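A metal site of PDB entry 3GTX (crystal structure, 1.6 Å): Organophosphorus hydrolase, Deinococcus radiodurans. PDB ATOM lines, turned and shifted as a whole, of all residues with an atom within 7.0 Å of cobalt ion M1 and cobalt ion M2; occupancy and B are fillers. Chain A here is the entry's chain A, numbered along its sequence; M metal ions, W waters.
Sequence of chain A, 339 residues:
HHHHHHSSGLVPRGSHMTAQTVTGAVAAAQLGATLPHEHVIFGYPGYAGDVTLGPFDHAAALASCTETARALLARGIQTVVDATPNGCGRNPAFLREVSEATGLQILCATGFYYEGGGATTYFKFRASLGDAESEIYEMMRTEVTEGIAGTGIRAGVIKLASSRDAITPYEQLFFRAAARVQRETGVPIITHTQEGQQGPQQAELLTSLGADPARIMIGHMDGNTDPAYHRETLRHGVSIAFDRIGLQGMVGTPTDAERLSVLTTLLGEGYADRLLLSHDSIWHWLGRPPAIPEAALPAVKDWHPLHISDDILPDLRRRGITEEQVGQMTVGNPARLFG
Cobalt ion M1 is bound by water W2 (1.7 Å), NE2 of His 39 (2.0 Å), OQ2 of KCX 159 (2.1 Å), NE2 of His 37 (2.1 Å) and OD1 of Asp 280 (2.2 Å).
The backbone NH of Asp 280 is in hydrogen-bond range of the backbone carbonyl oxygen of Asp 243. The side-chain hydroxyl (OG1) of Thr 193 lies within hydrogen-bond range of the backbone carbonyl oxygen (O) of His 220 (3.3 Å). A ring nitrogen (ND1) of His 39 sits at hydrogen-bond distance from the side-chain hydroxyl of Thr 84. The backbone carbonyl oxygen of Ala 83 sits close to NZ of KCX 159 (3.0 Å). The side-chain carboxylate of Asp 280 lies within salt-bridge range of the guanidinium group of Arg 244. The backbone carbonyl oxygen (O) of Ser 281 sits at hydrogen-bond distance from the backbone NH (N) of His 39 (2.9 Å). OE1 of Gln 194 lies within hydrogen-bond range of NE2 of His 192, 3.1 Å away. The side-chain carboxylate of Asp 243 lies within hydrogen-bond range of a ring nitrogen (ND1) of His 220, at 2.5 Å.
Cobalt ion M2 is bound by OQ1 of KCX 159 (2.1 Å), the side-chain hydroxyl of Tyr 113 (2.1 Å), a ring nitrogen (ND1) of His 192 (2.2 Å), a ring nitrogen (NE2) of His 220 (2.3 Å), water W2 (2.3 Å) and water W1 (2.4 Å). Cobalt ion M2 has six donor atoms within binding distance.
Within 4 Å of cobalt ion M1: His 37, His 39, KCX 159 and Asp 280. Along chain A the residues within 4 Å of cobalt ion M1 span positions 37 to 280. The nearest printed residue that does not touch cobalt ion M1 is Tyr 113 (4.3 Å).
Four residues have an atom within 4 Å of cobalt ion M2: Tyr 113, KCX 159, His 192 and His 220. The nearest printed residue that does not touch cobalt ion M2 is Asp 280 (4.2 Å).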
ATOM      1  N   HIS A  37       3.368 -16.367 -18.996  1.00  0.00           N
ATOM      2  CA  HIS A  37       2.598 -15.732 -20.023  1.00  0.00           C
ATOM      3  C   HIS A  37       1.765 -14.606 -19.292  1.00  0.00           C
ATOM      4  O   HIS A  37       0.723 -14.872 -18.743  1.00  0.00           O
ATOM      5  CB  HIS A  37       1.623 -16.719 -20.677  1.00  0.00           C
ATOM      6  CG  HIS A  37       0.865 -16.119 -21.800  1.00  0.00           C
ATOM      7  ND1 HIS A  37       0.964 -16.551 -23.123  1.00  0.00           N
ATOM      8  CD2 HIS A  37       0.047 -15.037 -21.827  1.00  0.00           C
ATOM      9  CE1 HIS A  37       0.246 -15.741 -23.901  1.00  0.00           C
ATOM     10  NE2 HIS A  37      -0.334 -14.825 -23.125  1.00  0.00           N
ATOM     11  N   GLU A  38       2.292 -13.418 -19.450  1.00  0.00           N
ATOM     12  CA  GLU A  38       1.672 -12.180 -18.867  1.00  0.00           C
ATOM     13  C   GLU A  38       1.907 -11.020 -19.836  1.00  0.00           C
ATOM     14  O   GLU A  38       2.645 -11.119 -20.821  1.00  0.00           O
ATOM     15  CB  GLU A  38       2.370 -11.896 -17.539  1.00  0.00           C
ATOM     16  CG  GLU A  38       2.252 -13.008 -16.395  1.00  0.00           C
ATOM     17  CD  GLU A  38       0.829 -13.433 -16.013  1.00  0.00           C
ATOM     18  OE1 GLU A  38      -0.071 -12.548 -16.069  1.00  0.00           O
ATOM     19  OE2 GLU A  38       0.587 -14.644 -15.661  1.00  0.00           O
ATOM     20  N   HIS A  39       1.227  -9.887 -19.615  1.00  0.00           N
ATOM     21  CA  HIS A  39       1.411  -8.732 -20.471  1.00  0.00           C
ATOM     22  C   HIS A  39       1.632  -7.473 -19.623  1.00  0.00           C
ATOM     23  O   HIS A  39       0.679  -7.024 -18.970  1.00  0.00           O
ATOM     24  CB  HIS A  39       0.192  -8.563 -21.345  1.00  0.00           C
ATOM     25  CG  HIS A  39      -0.001  -9.722 -22.292  1.00  0.00           C
ATOM     26  ND1 HIS A  39       0.779  -9.888 -23.442  1.00  0.00           N
ATOM     27  CD2 HIS A  39      -0.911 -10.718 -22.300  1.00  0.00           C
ATOM     28  CE1 HIS A  39       0.332 -10.945 -24.103  1.00  0.00           C
ATOM     29  NE2 HIS A  39      -0.690 -11.473 -23.439  1.00  0.00           N
ATOM     30  N   PHE A  42      -0.577  -3.831 -22.810  1.00  0.00           N
ATOM     31  CA  PHE A  42      -1.172  -4.483 -23.972  1.00  0.00           C
ATOM     32  C   PHE A  42      -2.277  -3.631 -24.580  1.00  0.00           C
ATOM     33  O   PHE A  42      -3.066  -2.994 -23.863  1.00  0.00           O
ATOM     34  CB  PHE A  42      -1.758  -5.833 -23.562  1.00  0.00           C
ATOM     35  CG  PHE A  42      -2.383  -6.595 -24.699  1.00  0.00           C
ATOM     36  CD1 PHE A  42      -3.704  -6.316 -25.088  1.00  0.00           C
ATOM     37  CD2 PHE A  42      -1.678  -7.635 -25.383  1.00  0.00           C
ATOM     38  CE1 PHE A  42      -4.365  -7.011 -26.112  1.00  0.00           C
ATOM     39  CE2 PHE A  42      -2.340  -8.356 -26.440  1.00  0.00           C
ATOM     40  CZ  PHE A  42      -3.702  -8.037 -26.800  1.00  0.00           C
ATOM     41  N   ALA A  83       4.391 -12.002 -23.103  1.00  0.00           N
ATOM     42  CA  ALA A  83       3.948 -12.674 -24.346  1.00  0.00           C
ATOM     43  C   ALA A  83       3.332 -11.735 -25.436  1.00  0.00           C
ATOM     44  O   ALA A  83       2.776 -12.176 -26.433  1.00  0.00           O
ATOM     45  CB  ALA A  83       2.953 -13.697 -23.966  1.00  0.00           C
ATOM     46  N   THR A  84       3.480 -10.425 -25.237  1.00  0.00           N
ATOM     47  CA  THR A  84       2.901  -9.456 -26.133  1.00  0.00           C
ATOM     48  C   THR A  84       3.467  -9.475 -27.540  1.00  0.00           C
ATOM     49  O   THR A  84       4.657  -9.198 -27.732  1.00  0.00           O
ATOM     50  CB  THR A  84       3.089  -8.011 -25.609  1.00  0.00           C
ATOM     51  OG1 THR A  84       2.748  -8.018 -24.214  1.00  0.00           O
ATOM     52  CG2 THR A  84       2.179  -7.009 -26.395  1.00  0.00           C
ATOM     53  N   PRO A  85       2.605  -9.703 -28.514  1.00  0.00           N
ATOM     54  CA  PRO A  85       2.992  -9.721 -29.927  1.00  0.00           C
ATOM     55  C   PRO A  85       3.408  -8.341 -30.425  1.00  0.00           C
ATOM     56  O   PRO A  85       3.070  -7.270 -29.849  1.00  0.00           O
ATOM     57  CB  PRO A  85       1.769 -10.225 -30.661  1.00  0.00           C
ATOM     58  CG  PRO A  85       0.924 -10.889 -29.619  1.00  0.00           C
ATOM     59  CD  PRO A  85       1.186 -10.081 -28.342  1.00  0.00           C
ATOM     60  N   TYR A 113       0.221 -11.801 -33.800  1.00  0.00           N
ATOM     61  CA  TYR A 113      -0.895 -12.558 -33.237  1.00  0.00           C
ATOM     62  C   TYR A 113      -1.638 -13.348 -34.274  1.00  0.00           C
ATOM     63  O   TYR A 113      -1.286 -13.331 -35.458  1.00  0.00           O
ATOM     64  CB  TYR A 113      -1.877 -11.607 -32.486  1.00  0.00           C
ATOM     65  CG  TYR A 113      -2.506 -12.142 -31.193  1.00  0.00           C
ATOM     66  CD1 TYR A 113      -1.964 -13.229 -30.507  1.00  0.00           C
ATOM     67  CD2 TYR A 113      -3.594 -11.454 -30.580  1.00  0.00           C
ATOM     68  CE1 TYR A 113      -2.447 -13.661 -29.236  1.00  0.00           C
ATOM     69  CE2 TYR A 113      -4.074 -11.869 -29.335  1.00  0.00           C
ATOM     70  CZ  TYR A 113      -3.498 -12.959 -28.674  1.00  0.00           C
ATOM     71  OH  TYR A 113      -3.913 -13.412 -27.488  1.00  0.00           O
ATOM     72  N   TYR A 114      -2.649 -14.080 -33.821  1.00  0.00           N
ATOM     73  CA  TYR A 114      -3.399 -14.921 -34.730  1.00  0.00           C
ATOM     74  C   TYR A 114      -4.130 -14.073 -35.770  1.00  0.00           C
ATOM     75  O   TYR A 114      -4.413 -12.915 -35.553  1.00  0.00           O
ATOM     76  CB  TYR A 114      -4.359 -15.863 -33.962  1.00  0.00           C
ATOM     77  CG  TYR A 114      -5.540 -15.196 -33.303  1.00  0.00           C
ATOM     78  CD1 TYR A 114      -5.394 -14.494 -32.116  1.00  0.00           C
ATOM     79  CD2 TYR A 114      -6.812 -15.292 -33.852  1.00  0.00           C
ATOM     80  CE1 TYR A 114      -6.502 -13.903 -31.483  1.00  0.00           C
ATOM     81  CE2 TYR A 114      -7.901 -14.688 -33.225  1.00  0.00           C
ATOM     82  CZ  TYR A 114      -7.731 -14.003 -32.059  1.00  0.00           C
ATOM     83  OH  TYR A 114      -8.811 -13.370 -31.477  1.00  0.00           O
ATOM     84  N   KCX A 159       6.843 -15.761 -29.995  1.00  0.00           N
ATOM     85  CA  KCX A 159       5.424 -15.957 -29.709  1.00  0.00           C
ATOM     86  CB  KCX A 159       4.808 -14.615 -29.098  1.00  0.00           C
ATOM     87  CG  KCX A 159       3.220 -14.625 -29.101  1.00  0.00           C
ATOM     88  CD  KCX A 159       2.574 -15.566 -28.078  1.00  0.00           C
ATOM     89  CE  KCX A 159       1.066 -15.434 -27.941  1.00  0.00           C
ATOM     90  NZ  KCX A 159       0.732 -14.292 -27.079  1.00  0.00           N
ATOM     91  C   KCX A 159       4.670 -16.327 -31.000  1.00  0.00           C
ATOM     92  O   KCX A 159       4.682 -15.562 -31.984  1.00  0.00           O
ATOM     93  CX  KCX A 159      -0.444 -14.067 -26.504  1.00  0.00           C
ATOM     94  OQ1 KCX A 159      -1.379 -14.899 -26.522  1.00  0.00           O
ATOM     95  OQ2 KCX A 159      -0.586 -13.047 -25.786  1.00  0.00           O
ATOM     96  N   ALA A 161       0.751 -17.896 -32.655  1.00  0.00           N
ATOM     97  CA  ALA A 161      -0.651 -17.985 -32.367  1.00  0.00           C
ATOM     98  C   ALA A 161      -1.462 -18.496 -33.545  1.00  0.00           C
ATOM     99  O   ALA A 161      -1.218 -18.136 -34.695  1.00  0.00           O
ATOM    100  CB  ALA A 161      -1.162 -16.591 -31.975  1.00  0.00           C
ATOM    101  N   THR A 191       3.102 -20.383 -27.274  1.00  0.00           N
ATOM    102  CA  THR A 191       1.975 -20.176 -28.129  1.00  0.00           C
ATOM    103  C   THR A 191       0.671 -19.720 -27.498  1.00  0.00           C
ATOM    104  O   THR A 191       0.523 -19.758 -26.254  1.00  0.00           O
ATOM    105  CB  THR A 191       1.626 -21.406 -28.988  1.00  0.00           C
ATOM    106  OG1 THR A 191       0.717 -22.248 -28.311  1.00  0.00           O
ATOM    107  CG2 THR A 191       2.908 -22.153 -29.323  1.00  0.00           C
ATOM    108  N   HIS A 192      -0.242 -19.322 -28.401  1.00  0.00           N
ATOM    109  CA  HIS A 192      -1.608 -18.922 -28.146  1.00  0.00           C
ATOM    110  C   HIS A 192      -2.480 -19.920 -28.912  1.00  0.00           C
ATOM    111  O   HIS A 192      -2.267 -20.153 -30.098  1.00  0.00           O
ATOM    112  CB  HIS A 192      -1.896 -17.549 -28.766  1.00  0.00           C
ATOM    113  CG  HIS A 192      -3.358 -17.255 -28.928  1.00  0.00           C
ATOM    114  ND1 HIS A 192      -4.016 -16.329 -28.137  1.00  0.00           N
ATOM    115  CD2 HIS A 192      -4.261 -17.629 -29.875  1.00  0.00           C
ATOM    116  CE1 HIS A 192      -5.241 -16.127 -28.611  1.00  0.00           C
ATOM    117  NE2 HIS A 192      -5.407 -16.897 -29.676  1.00  0.00           N
ATOM    118  N   THR A 193      -3.512 -20.460 -28.280  1.00  0.00           N
ATOM    119  CA  THR A 193      -4.486 -21.278 -28.997  1.00  0.00           C
ATOM    120  C   THR A 193      -5.769 -20.511 -28.814  1.00  0.00           C
ATOM    121  O   THR A 193      -5.954 -19.851 -27.783  1.00  0.00           O
ATOM    122  CB  THR A 193      -4.664 -22.692 -28.432  1.00  0.00           C
ATOM    123  OG1 THR A 193      -4.909 -22.651 -26.999  1.00  0.00           O
ATOM    124  CG2 THR A 193      -3.408 -23.490 -28.774  1.00  0.00           C
ATOM    125  N   GLN A 194      -6.665 -20.609 -29.783  1.00  0.00           N
ATOM    126  CA  GLN A 194      -7.901 -19.859 -29.754  1.00  0.00           C
ATOM    127  C   GLN A 194      -9.067 -20.721 -29.414  1.00  0.00           C
ATOM    128  O   GLN A 194      -9.297 -21.696 -30.093  1.00  0.00           O
ATOM    129  CB  GLN A 194      -8.077 -19.239 -31.137  1.00  0.00           C
ATOM    130  CG  GLN A 194      -9.357 -18.513 -31.360  1.00  0.00           C
ATOM    131  CD  GLN A 194      -9.429 -17.253 -30.513  1.00  0.00           C
ATOM    132  OE1 GLN A 194      -8.404 -16.632 -30.192  1.00  0.00           O
ATOM    133  NE2 GLN A 194     -10.637 -16.858 -30.185  1.00  0.00           N
ATOM    134  N   HIS A 220      -2.705 -21.306 -23.613  1.00  0.00           N
ATOM    135  CA  HIS A 220      -4.158 -21.297 -23.481  1.00  0.00           C
ATOM    136  C   HIS A 220      -4.847 -22.678 -23.521  1.00  0.00           C
ATOM    137  O   HIS A 220      -5.993 -22.816 -23.915  1.00  0.00           O
ATOM    138  CB  HIS A 220      -4.844 -20.344 -24.492  1.00  0.00           C
ATOM    139  CG  HIS A 220      -4.211 -18.994 -24.566  1.00  0.00           C
ATOM    140  ND1 HIS A 220      -3.436 -18.486 -23.547  1.00  0.00           N
ATOM    141  CD2 HIS A 220      -4.207 -18.034 -25.539  1.00  0.00           C
ATOM    142  CE1 HIS A 220      -2.983 -17.290 -23.887  1.00  0.00           C
ATOM    143  NE2 HIS A 220      -3.435 -17.004 -25.084  1.00  0.00           N
ATOM    144  N   ASP A 243      -2.712 -20.881 -18.816  1.00  0.00           N
ATOM    145  CA  ASP A 243      -2.143 -19.550 -18.644  1.00  0.00           C
ATOM    146  C   ASP A 243      -3.125 -18.368 -18.681  1.00  0.00           C
ATOM    147  O   ASP A 243      -2.684 -17.235 -18.873  1.00  0.00           O
ATOM    148  CB  ASP A 243      -1.007 -19.311 -19.650  1.00  0.00           C
ATOM    149  CG  ASP A 243      -1.445 -19.555 -21.130  1.00  0.00           C
ATOM    150  OD1 ASP A 243      -2.667 -19.534 -21.421  1.00  0.00           O
ATOM    151  OD2 ASP A 243      -0.561 -19.765 -21.992  1.00  0.00           O
ATOM    152  N   ARG A 244      -4.402 -18.638 -18.539  1.00  0.00           N
ATOM    153  CA  ARG A 244      -5.437 -17.557 -18.486  1.00  0.00           C
ATOM    154  C   ARG A 244      -6.192 -17.734 -17.156  1.00  0.00           C
ATOM    155  O   ARG A 244      -7.382 -17.440 -17.065  1.00  0.00           O
ATOM    156  CB  ARG A 244      -6.416 -17.644 -19.670  1.00  0.00           C
ATOM    157  CG  ARG A 244      -5.680 -17.734 -21.020  1.00  0.00           C
ATOM    158  CD  ARG A 244      -6.555 -17.410 -22.170  1.00  0.00           C
ATOM    159  NE  ARG A 244      -6.744 -15.979 -22.321  1.00  0.00           N
ATOM    160  CZ  ARG A 244      -7.762 -15.489 -22.998  1.00  0.00           C
ATOM    161  NH1 ARG A 244      -8.636 -16.325 -23.548  1.00  0.00           N
ATOM    162  NH2 ARG A 244      -7.900 -14.184 -23.130  1.00  0.00           N
ATOM    163  N   ASP A 280      -2.259 -14.525 -18.014  1.00  0.00           N
ATOM    164  CA  ASP A 280      -2.494 -13.798 -19.261  1.00  0.00           C
ATOM    165  C   ASP A 280      -3.084 -12.436 -18.847  1.00  0.00           C
ATOM    166  O   ASP A 280      -3.918 -11.892 -19.543  1.00  0.00           O
ATOM    167  CB  ASP A 280      -3.460 -14.525 -20.181  1.00  0.00           C
ATOM    168  CG  ASP A 280      -3.432 -13.969 -21.601  1.00  0.00           C
ATOM    169  OD1 ASP A 280      -2.449 -13.295 -21.962  1.00  0.00           O
ATOM    170  OD2 ASP A 280      -4.371 -14.134 -22.353  1.00  0.00           O
ATOM    171  N   SER A 281      -2.583 -11.898 -17.736  1.00  0.00           N
ATOM    172  CA  SER A 281      -3.135 -10.595 -17.288  1.00  0.00           C
ATOM    173  C   SER A 281      -2.536  -9.414 -18.050  1.00  0.00           C
ATOM    174  O   SER A 281      -1.499  -9.531 -18.726  1.00  0.00           O
ATOM    175  CB  SER A 281      -2.857 -10.421 -15.808  1.00  0.00           C
ATOM    176  OG  SER A 281      -1.444 -10.336 -15.561  1.00  0.00           O
ATOM    177  N   ILE A 282      -3.164  -8.236 -17.910  1.00  0.00           N
ATOM    178  CA  ILE A 282      -2.677  -7.056 -18.593  1.00  0.00           C
ATOM    179  C   ILE A 282      -2.506  -6.074 -17.442  1.00  0.00           C
ATOM    180  O   ILE A 282      -3.484  -5.806 -16.769  1.00  0.00           O
ATOM    181  CB  ILE A 282      -3.683  -6.562 -19.617  1.00  0.00           C
ATOM    182  CG1 ILE A 282      -3.689  -7.545 -20.811  1.00  0.00           C
ATOM    183  CG2 ILE A 282      -3.315  -5.222 -20.057  1.00  0.00           C
ATOM    184  CD1 ILE A 282      -4.814  -7.318 -21.766  1.00  0.00           C
HETATM  185 CO    CO M   1      -1.493 -13.224 -23.941  1.00  0.00          CO
HETATM  186 CO    CO M   2      -3.429 -15.138 -26.352  1.00  0.00          CO
HETATM  187  O   HOH W   1      -5.740 -15.097 -25.772  1.00  0.00           O
HETATM  188  O   HOH W   2      -2.985 -13.841 -24.539  1.00  0.00           O
